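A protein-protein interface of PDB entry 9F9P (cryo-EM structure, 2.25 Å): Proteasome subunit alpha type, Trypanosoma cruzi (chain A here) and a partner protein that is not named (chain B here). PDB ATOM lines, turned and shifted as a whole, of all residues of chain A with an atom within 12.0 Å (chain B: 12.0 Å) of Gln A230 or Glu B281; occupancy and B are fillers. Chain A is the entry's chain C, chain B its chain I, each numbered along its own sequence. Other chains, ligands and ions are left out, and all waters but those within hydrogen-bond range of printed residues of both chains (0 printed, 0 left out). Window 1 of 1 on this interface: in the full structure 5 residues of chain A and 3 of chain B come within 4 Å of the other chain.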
ATOM      1  N   ALA A 226      10.072  16.683  -0.078  1.00  0.00           N
ATOM      2  CA  ALA A 226      11.297  17.467  -0.131  1.00  0.00           C
ATOM      3  C   ALA A 226      12.117  17.055  -1.356  1.00  0.00           C
ATOM      4  O   ALA A 226      12.014  15.917  -1.814  1.00  0.00           O
ATOM      5  CB  ALA A 226      12.052  17.307   1.170  1.00  0.00           C
ATOM      6  N   PRO A 227      12.935  17.960  -1.949  1.00  0.00           N
ATOM      7  CA  PRO A 227      13.676  17.639  -3.177  1.00  0.00           C
ATOM      8  C   PRO A 227      15.008  16.931  -2.891  1.00  0.00           C
ATOM      9  O   PRO A 227      15.057  16.007  -2.081  1.00  0.00           O
ATOM     10  CB  PRO A 227      13.781  19.047  -3.801  1.00  0.00           C
ATOM     11  CG  PRO A 227      14.000  19.966  -2.605  1.00  0.00           C
ATOM     12  CD  PRO A 227      13.185  19.340  -1.487  1.00  0.00           C
ATOM     13  N   ALA A 228      16.081  17.359  -3.577  1.00  0.00           N
ATOM     14  CA  ALA A 228      17.438  16.873  -3.349  1.00  0.00           C
ATOM     15  C   ALA A 228      17.767  16.834  -1.854  1.00  0.00           C
ATOM     16  O   ALA A 228      17.114  17.485  -1.039  1.00  0.00           O
ATOM     17  CB  ALA A 228      18.428  17.755  -4.086  1.00  0.00           C
ATOM     18  N   THR A 229      18.809  16.069  -1.515  1.00  0.00           N
ATOM     19  CA  THR A 229      19.375  16.040  -0.175  1.00  0.00           C
ATOM     20  C   THR A 229      20.888  15.867  -0.300  1.00  0.00           C
ATOM     21  O   THR A 229      21.413  14.787  -0.036  1.00  0.00           O
ATOM     22  CB  THR A 229      18.701  14.954   0.680  1.00  0.00           C
ATOM     23  OG1 THR A 229      18.000  14.069  -0.195  1.00  0.00           O
ATOM     24  CG2 THR A 229      17.730  15.514   1.697  1.00  0.00           C
ATOM     25  N   GLN A 230      21.575  16.942  -0.713  1.00  0.00           N
ATOM     26  CA  GLN A 230      22.980  16.869  -1.091  1.00  0.00           C
ATOM     27  C   GLN A 230      23.844  16.775   0.165  1.00  0.00           C
ATOM     28  O   GLN A 230      24.273  17.797   0.685  1.00  0.00           O
ATOM     29  CB  GLN A 230      23.421  18.102  -1.883  1.00  0.00           C
ATOM     30  CG  GLN A 230      22.476  18.527  -2.997  1.00  0.00           C
ATOM     31  CD  GLN A 230      22.280  20.025  -2.949  1.00  0.00           C
ATOM     32  OE1 GLN A 230      21.847  20.582  -1.940  1.00  0.00           O
ATOM     33  NE2 GLN A 230      22.625  20.700  -4.032  1.00  0.00           N
ATOM     34  N   LYS A 231      24.111  15.550   0.635  1.00  0.00           N
ATOM     35  CA  LYS A 231      24.917  15.338   1.825  1.00  0.00           C
ATOM     36  C   LYS A 231      26.408  15.356   1.490  1.00  0.00           C
ATOM     37  O   LYS A 231      27.248  15.228   2.382  1.00  0.00           O
ATOM     38  CB  LYS A 231      24.541  14.021   2.516  1.00  0.00           C
ATOM     39  CG  LYS A 231      23.236  14.061   3.300  1.00  0.00           C
ATOM     40  CD  LYS A 231      22.505  12.731   3.312  1.00  0.00           C
ATOM     41  CE  LYS A 231      21.000  12.881   3.414  1.00  0.00           C
ATOM     42  NZ  LYS A 231      20.300  11.623   3.061  1.00  0.00           N
ATOM     43  N   LEU A 232      26.745  15.519   0.214  1.00  0.00           N
ATOM     44  CA  LEU A 232      28.135  15.650  -0.185  1.00  0.00           C
ATOM     45  C   LEU A 232      28.564  17.108  -0.100  1.00  0.00           C
ATOM     46  O   LEU A 232      29.701  17.367   0.287  1.00  0.00           O
ATOM     47  CB  LEU A 232      28.329  15.077  -1.596  1.00  0.00           C
ATOM     48  CG  LEU A 232      28.091  13.568  -1.689  1.00  0.00           C
ATOM     49  CD1 LEU A 232      28.585  12.981  -3.016  1.00  0.00           C
ATOM     50  CD2 LEU A 232      28.736  12.863  -0.507  1.00  0.00           C
ATOM     51  N   LEU A 233      27.667  18.030  -0.475  1.00  0.00           N
ATOM     52  CA  LEU A 233      27.940  19.459  -0.395  1.00  0.00           C
ATOM     53  C   LEU A 233      27.545  20.032   0.975  1.00  0.00           C
ATOM     54  O   LEU A 233      28.200  20.952   1.446  1.00  0.00           O
ATOM     55  CB  LEU A 233      27.256  20.160  -1.573  1.00  0.00           C
ATOM     56  CG  LEU A 233      27.665  19.638  -2.959  1.00  0.00           C
ATOM     57  CD1 LEU A 233      26.949  20.365  -4.087  1.00  0.00           C
ATOM     58  CD2 LEU A 233      29.157  19.764  -3.188  1.00  0.00           C
ATOM     59  N   GLU A 234      26.520  19.491   1.650  1.00  0.00           N
ATOM     60  CA  GLU A 234      26.184  19.911   3.009  1.00  0.00           C
ATOM     61  C   GLU A 234      26.184  18.721   3.968  1.00  0.00           C
ATOM     62  O   GLU A 234      25.127  18.243   4.359  1.00  0.00           O
ATOM     63  CB  GLU A 234      24.819  20.603   3.086  1.00  0.00           C
ATOM     64  CG  GLU A 234      24.823  22.051   2.624  1.00  0.00           C
ATOM     65  CD  GLU A 234      24.295  22.307   1.219  1.00  0.00           C
ATOM     66  OE1 GLU A 234      23.090  22.034   0.976  1.00  0.00           O
ATOM     67  OE2 GLU A 234      25.085  22.802   0.376  1.00  0.00           O
ATOM     68  N   PRO A 235      27.360  18.247   4.426  1.00  0.00           N
ATOM     69  CA  PRO A 235      27.449  17.091   5.322  1.00  0.00           C
ATOM     70  C   PRO A 235      26.696  17.113   6.654  1.00  0.00           C
ATOM     71  O   PRO A 235      26.603  16.084   7.307  1.00  0.00           O
ATOM     72  CB  PRO A 235      28.946  17.043   5.678  1.00  0.00           C
ATOM     73  CG  PRO A 235      29.638  17.707   4.518  1.00  0.00           C
ATOM     74  CD  PRO A 235      28.685  18.808   4.103  1.00  0.00           C
ATOM     75  N   TYR A 236      26.228  18.288   7.092  1.00  0.00           N
ATOM     76  CA  TYR A 236      25.447  18.396   8.321  1.00  0.00           C
ATOM     77  C   TYR A 236      24.061  18.990   8.065  1.00  0.00           C
ATOM     78  O   TYR A 236      23.328  19.254   9.016  1.00  0.00           O
ATOM     79  CB  TYR A 236      26.198  19.251   9.343  1.00  0.00           C
ATOM     80  CG  TYR A 236      27.403  18.592   9.953  1.00  0.00           C
ATOM     81  CD1 TYR A 236      27.291  17.813  11.098  1.00  0.00           C
ATOM     82  CD2 TYR A 236      28.656  18.732   9.372  1.00  0.00           C
ATOM     83  CE1 TYR A 236      28.404  17.200  11.670  1.00  0.00           C
ATOM     84  CE2 TYR A 236      29.770  18.112   9.921  1.00  0.00           C
ATOM     85  CZ  TYR A 236      29.645  17.341  11.073  1.00  0.00           C
ATOM     86  OH  TYR A 236      30.760  16.744  11.609  1.00  0.00           O
ATOM     87  N   GLY A 237      23.698  19.177   6.785  1.00  0.00           N
ATOM     88  CA  GLY A 237      22.359  19.617   6.415  1.00  0.00           C
ATOM     89  C   GLY A 237      21.312  18.520   6.617  1.00  0.00           C
ATOM     90  O   GLY A 237      21.512  17.388   6.199  1.00  0.00           O
ATOM     91  N   VAL A 238      20.201  18.871   7.277  1.00  0.00           N
ATOM     92  CA  VAL A 238      19.099  17.948   7.519  1.00  0.00           C
ATOM     93  C   VAL A 238      17.814  18.621   7.048  1.00  0.00           C
ATOM     94  O   VAL A 238      17.417  19.630   7.625  1.00  0.00           O
ATOM     95  CB  VAL A 238      18.995  17.547   9.009  1.00  0.00           C
ATOM     96  CG1 VAL A 238      17.939  16.469   9.232  1.00  0.00           C
ATOM     97  CG2 VAL A 238      20.332  17.101   9.592  1.00  0.00           C
ATOM     98  N   LEU A 239      17.191  18.066   5.996  1.00  0.00           N
ATOM     99  CA  LEU A 239      15.837  18.433   5.596  1.00  0.00           C
ATOM    100  C   LEU A 239      14.849  17.444   6.207  1.00  0.00           C
ATOM    101  O   LEU A 239      15.242  16.340   6.576  1.00  0.00           O
ATOM    102  CB  LEU A 239      15.716  18.429   4.066  1.00  0.00           C
ATOM    103  CG  LEU A 239      16.320  19.624   3.319  1.00  0.00           C
ATOM    104  CD1 LEU A 239      16.002  19.536   1.830  1.00  0.00           C
ATOM    105  CD2 LEU A 239      15.832  20.956   3.887  1.00  0.00           C
ATOM    106  N   PRO A 240      13.548  17.804   6.348  1.00  0.00           N
ATOM    107  CA  PRO A 240      12.487  16.831   6.644  1.00  0.00           C
ATOM    108  C   PRO A 240      11.909  16.182   5.378  1.00  0.00           C
ATOM    109  O   PRO A 240      12.387  16.433   4.274  1.00  0.00           O
ATOM    110  CB  PRO A 240      11.436  17.672   7.399  1.00  0.00           C
ATOM    111  CG  PRO A 240      11.964  19.112   7.393  1.00  0.00           C
ATOM    112  CD  PRO A 240      13.016  19.174   6.306  1.00  0.00           C
ATOM    113  N   VAL A 243       8.092  19.723   2.614  1.00  0.00           N
ATOM    114  CA  VAL A 243       8.312  21.168   2.722  1.00  0.00           C
ATOM    115  C   VAL A 243       7.091  21.904   2.196  1.00  0.00           C
ATOM    116  O   VAL A 243       6.540  21.516   1.177  1.00  0.00           O
ATOM    117  CB  VAL A 243       9.570  21.631   1.957  1.00  0.00           C
ATOM    118  CG1 VAL A 243      10.809  20.944   2.490  1.00  0.00           C
ATOM    119  CG2 VAL A 243       9.477  21.380   0.457  1.00  0.00           C
ATOM    120  N   VAL B 277      36.513   6.761  -6.279  1.00  0.00           N
ATOM    121  CA  VAL B 277      35.349   7.484  -5.791  1.00  0.00           C
ATOM    122  C   VAL B 277      34.773   6.701  -4.610  1.00  0.00           C
ATOM    123  O   VAL B 277      34.758   5.471  -4.645  1.00  0.00           O
ATOM    124  CB  VAL B 277      34.319   7.665  -6.928  1.00  0.00           C
ATOM    125  CG1 VAL B 277      32.971   8.151  -6.416  1.00  0.00           C
ATOM    126  CG2 VAL B 277      34.832   8.581  -8.036  1.00  0.00           C
ATOM    127  N   LEU B 278      34.300   7.418  -3.574  1.00  0.00           N
ATOM    128  CA  LEU B 278      33.706   6.800  -2.393  1.00  0.00           C
ATOM    129  C   LEU B 278      32.176   6.815  -2.460  1.00  0.00           C
ATOM    130  O   LEU B 278      31.546   5.893  -1.948  1.00  0.00           O
ATOM    131  CB  LEU B 278      34.186   7.519  -1.123  1.00  0.00           C
ATOM    132  CG  LEU B 278      35.687   7.460  -0.814  1.00  0.00           C
ATOM    133  CD1 LEU B 278      36.070   8.469   0.277  1.00  0.00           C
ATOM    134  CD2 LEU B 278      36.121   6.045  -0.425  1.00  0.00           C
ATOM    135  N   ARG B 279      31.577   7.869  -3.046  1.00  0.00           N
ATOM    136  CA  ARG B 279      30.130   8.073  -3.009  1.00  0.00           C
ATOM    137  C   ARG B 279      29.673   8.934  -4.185  1.00  0.00           C
ATOM    138  O   ARG B 279      30.465   9.657  -4.787  1.00  0.00           O
ATOM    139  CB  ARG B 279      29.658   8.787  -1.736  1.00  0.00           C
ATOM    140  CG  ARG B 279      29.869   8.040  -0.430  1.00  0.00           C
ATOM    141  CD  ARG B 279      28.844   8.485   0.602  1.00  0.00           C
ATOM    142  NE  ARG B 279      29.447   8.726   1.907  1.00  0.00           N
ATOM    143  CZ  ARG B 279      29.362   9.872   2.580  1.00  0.00           C
ATOM    144  NH1 ARG B 279      28.595  10.855   2.138  1.00  0.00           N
ATOM    145  NH2 ARG B 279      30.034  10.028   3.711  1.00  0.00           N
ATOM    146  N   GLU B 280      28.362   8.867  -4.456  1.00  0.00           N
ATOM    147  CA  GLU B 280      27.758   9.480  -5.629  1.00  0.00           C
ATOM    148  C   GLU B 280      26.282   9.786  -5.352  1.00  0.00           C
ATOM    149  O   GLU B 280      25.569   8.962  -4.778  1.00  0.00           O
ATOM    150  CB  GLU B 280      27.961   8.568  -6.844  1.00  0.00           C
ATOM    151  CG  GLU B 280      27.381   9.114  -8.143  1.00  0.00           C
ATOM    152  CD  GLU B 280      27.937   8.483  -9.412  1.00  0.00           C
ATOM    153  OE1 GLU B 280      29.106   8.769  -9.745  1.00  0.00           O
ATOM    154  OE2 GLU B 280      27.209   7.687 -10.059  1.00  0.00           O
ATOM    155  N   GLU B 281      25.848  11.003  -5.733  1.00  0.00           N
ATOM    156  CA  GLU B 281      24.437  11.376  -5.780  1.00  0.00           C
ATOM    157  C   GLU B 281      24.098  11.922  -7.170  1.00  0.00           C
ATOM    158  O   GLU B 281      24.938  12.565  -7.805  1.00  0.00           O
ATOM    159  CB  GLU B 281      24.096  12.428  -4.724  1.00  0.00           C
ATOM    160  CG  GLU B 281      24.310  11.965  -3.294  1.00  0.00           C
ATOM    161  CD  GLU B 281      24.031  13.038  -2.247  1.00  0.00           C
ATOM    162  OE1 GLU B 281      24.636  14.142  -2.345  1.00  0.00           O
ATOM    163  OE2 GLU B 281      23.209  12.777  -1.331  1.00  0.00           O
ATOM    164  N   ILE B 282      22.851  11.665  -7.612  1.00  0.00           N
ATOM    165  CA  ILE B 282      22.342  12.105  -8.909  1.00  0.00           C
ATOM    166  C   ILE B 282      21.053  12.908  -8.711  1.00  0.00           C
ATOM    167  O   ILE B 282      20.339  12.726  -7.722  1.00  0.00           O
ATOM    168  CB  ILE B 282      22.156  10.912  -9.877  1.00  0.00           C
ATOM    169  CG1 ILE B 282      23.390   9.998  -9.883  1.00  0.00           C
ATOM    170  CG2 ILE B 282      21.790  11.389 -11.279  1.00  0.00           C
ATOM    171  CD1 ILE B 282      23.717   9.335 -11.213  1.00  0.00           C
ATOM    172  N   ARG B 283      20.793  13.829  -9.650  1.00  0.00           N
ATOM    173  CA  ARG B 283      19.593  14.652  -9.634  1.00  0.00           C
ATOM    174  C   ARG B 283      19.196  15.008 -11.072  1.00  0.00           C
ATOM    175  O   ARG B 283      20.026  15.468 -11.853  1.00  0.00           O
ATOM    176  CB  ARG B 283      19.834  15.872  -8.735  1.00  0.00           C
ATOM    177  CG  ARG B 283      18.814  16.993  -8.891  1.00  0.00           C
ATOM    178  CD  ARG B 283      18.746  17.926  -7.696  1.00  0.00           C
ATOM    179  NE  ARG B 283      20.059  18.287  -7.166  1.00  0.00           N
ATOM    180  CZ  ARG B 283      20.535  19.526  -7.066  1.00  0.00           C
ATOM    181  NH1 ARG B 283      19.816  20.557  -7.476  1.00  0.00           N
ATOM    182  NH2 ARG B 283      21.739  19.726  -6.556  1.00  0.00           N
ATOM    183  N   ARG B 284      17.913  14.778 -11.404  1.00  0.00           N
ATOM    184  CA  ARG B 284      17.327  15.136 -12.691  1.00  0.00           C
ATOM    185  C   ARG B 284      16.706  16.532 -12.607  1.00  0.00           C
ATOM    186  O   ARG B 284      16.200  16.919 -11.552  1.00  0.00           O
ATOM    187  CB  ARG B 284      16.249  14.124 -13.093  1.00  0.00           C
ATOM    188  CG  ARG B 284      16.728  12.680 -13.143  1.00  0.00           C
ATOM    189  CD  ARG B 284      17.534  12.358 -14.388  1.00  0.00           C
ATOM    190  NE  ARG B 284      18.397  11.201 -14.174  1.00  0.00           N
ATOM    191  CZ  ARG B 284      19.076  10.571 -15.128  1.00  0.00           C
ATOM    192  NH1 ARG B 284      18.902  10.898 -16.396  1.00  0.00           N
ATOM    193  NH2 ARG B 284      19.909   9.594 -14.809  1.00  0.00           N
ATOM    194  N   LEU B 285      16.708  17.257 -13.738  1.00  0.00           N
ATOM    195  CA  LEU B 285      16.447  18.693 -13.762  1.00  0.00           C
ATOM    196  C   LEU B 285      15.098  18.990 -14.442  1.00  0.00           C
ATOM    197  O   LEU B 285      14.910  18.556 -15.600  1.00  0.00           O
ATOM    198  CB  LEU B 285      17.620  19.394 -14.469  1.00  0.00           C
ATOM    199  CG  LEU B 285      19.003  19.248 -13.814  1.00  0.00           C
ATOM    200  CD1 LEU B 285      20.061  20.050 -14.561  1.00  0.00           C
ATOM    201  CD2 LEU B 285      19.005  19.658 -12.344  1.00  0.00           C
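Hydrophobic or aromatic side chains of chain A within 4 Å of the printed part of chain B: Ala A228 and Leu A232. Among the printed residues, no Asp or Glu carboxylate lies within 4 Å of a Lys or Arg side-chain nitrogen of the other chain.
The side-chain carboxylate (OE1) of Glu B281 is in hydrogen-bond range of the backbone NH (N) of Lys A231, at 3.3 Å. NE2 of Gln A230 lies close to NH2 of Arg B283, at 2.8 Å. The backbone carbonyl oxygen (O) of Thr A229 sits close to the side-chain carboxylate (OE2) of Glu B281 (3.0 Å).
CB of Ala A228 touches NE of Arg B283 (3.5 Å). Glu B281 touches Gln A230 (OE1 to CA, 3.4 Å). Arg B279 touches Leu A232. CG of Leu A232 touches OE1 of Glu B281, 3.6 Å away.
The side-chain amide oxygen (OE1) of Gln A230 lies close to the side-chain carboxylate (OE1) of Glu A234.
Of chain B, only Glu B281 and Arg B283 come within 4 Å of Gln A230. Of chain A, only Thr A229 (3.0 Å), Gln A230 (3.4 Å), Lys A231 (3.3 Å) and Leu A232 (3.6 Å) come within 4 Å of Glu B281. Ala A228 touches just one residue of chain B: Arg B283 (3.5 Å). Thr A229 touches one residue of chain B. Of chain B, only Glu B281 comes within 4 Å of Lys A231. Of chain B, only Arg B279 and Glu B281 come within 4 Å of Leu A232. No residue of chain B comes within 4 Å of Glu A234. Pro A235 touches none of the printed residues of chain B. Gly A237 touches none of the printed residues of chain B. No residue of chain A comes within 4 Å of Glu B280. Of chain A, only Ala A228 and Gln A230 come within 4 Å of Arg B283. Printed residues of chain A within 4 Å of Arg B279: Leu A232. Pro A240 touches none of the printed residues of chain B. The nearest residue of chain B that does not touch Gln A230 is Ile B282 (7.8 Å). The nearest residue of chain A that does not touch Glu B281 is Leu A233 (5.3 Å).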
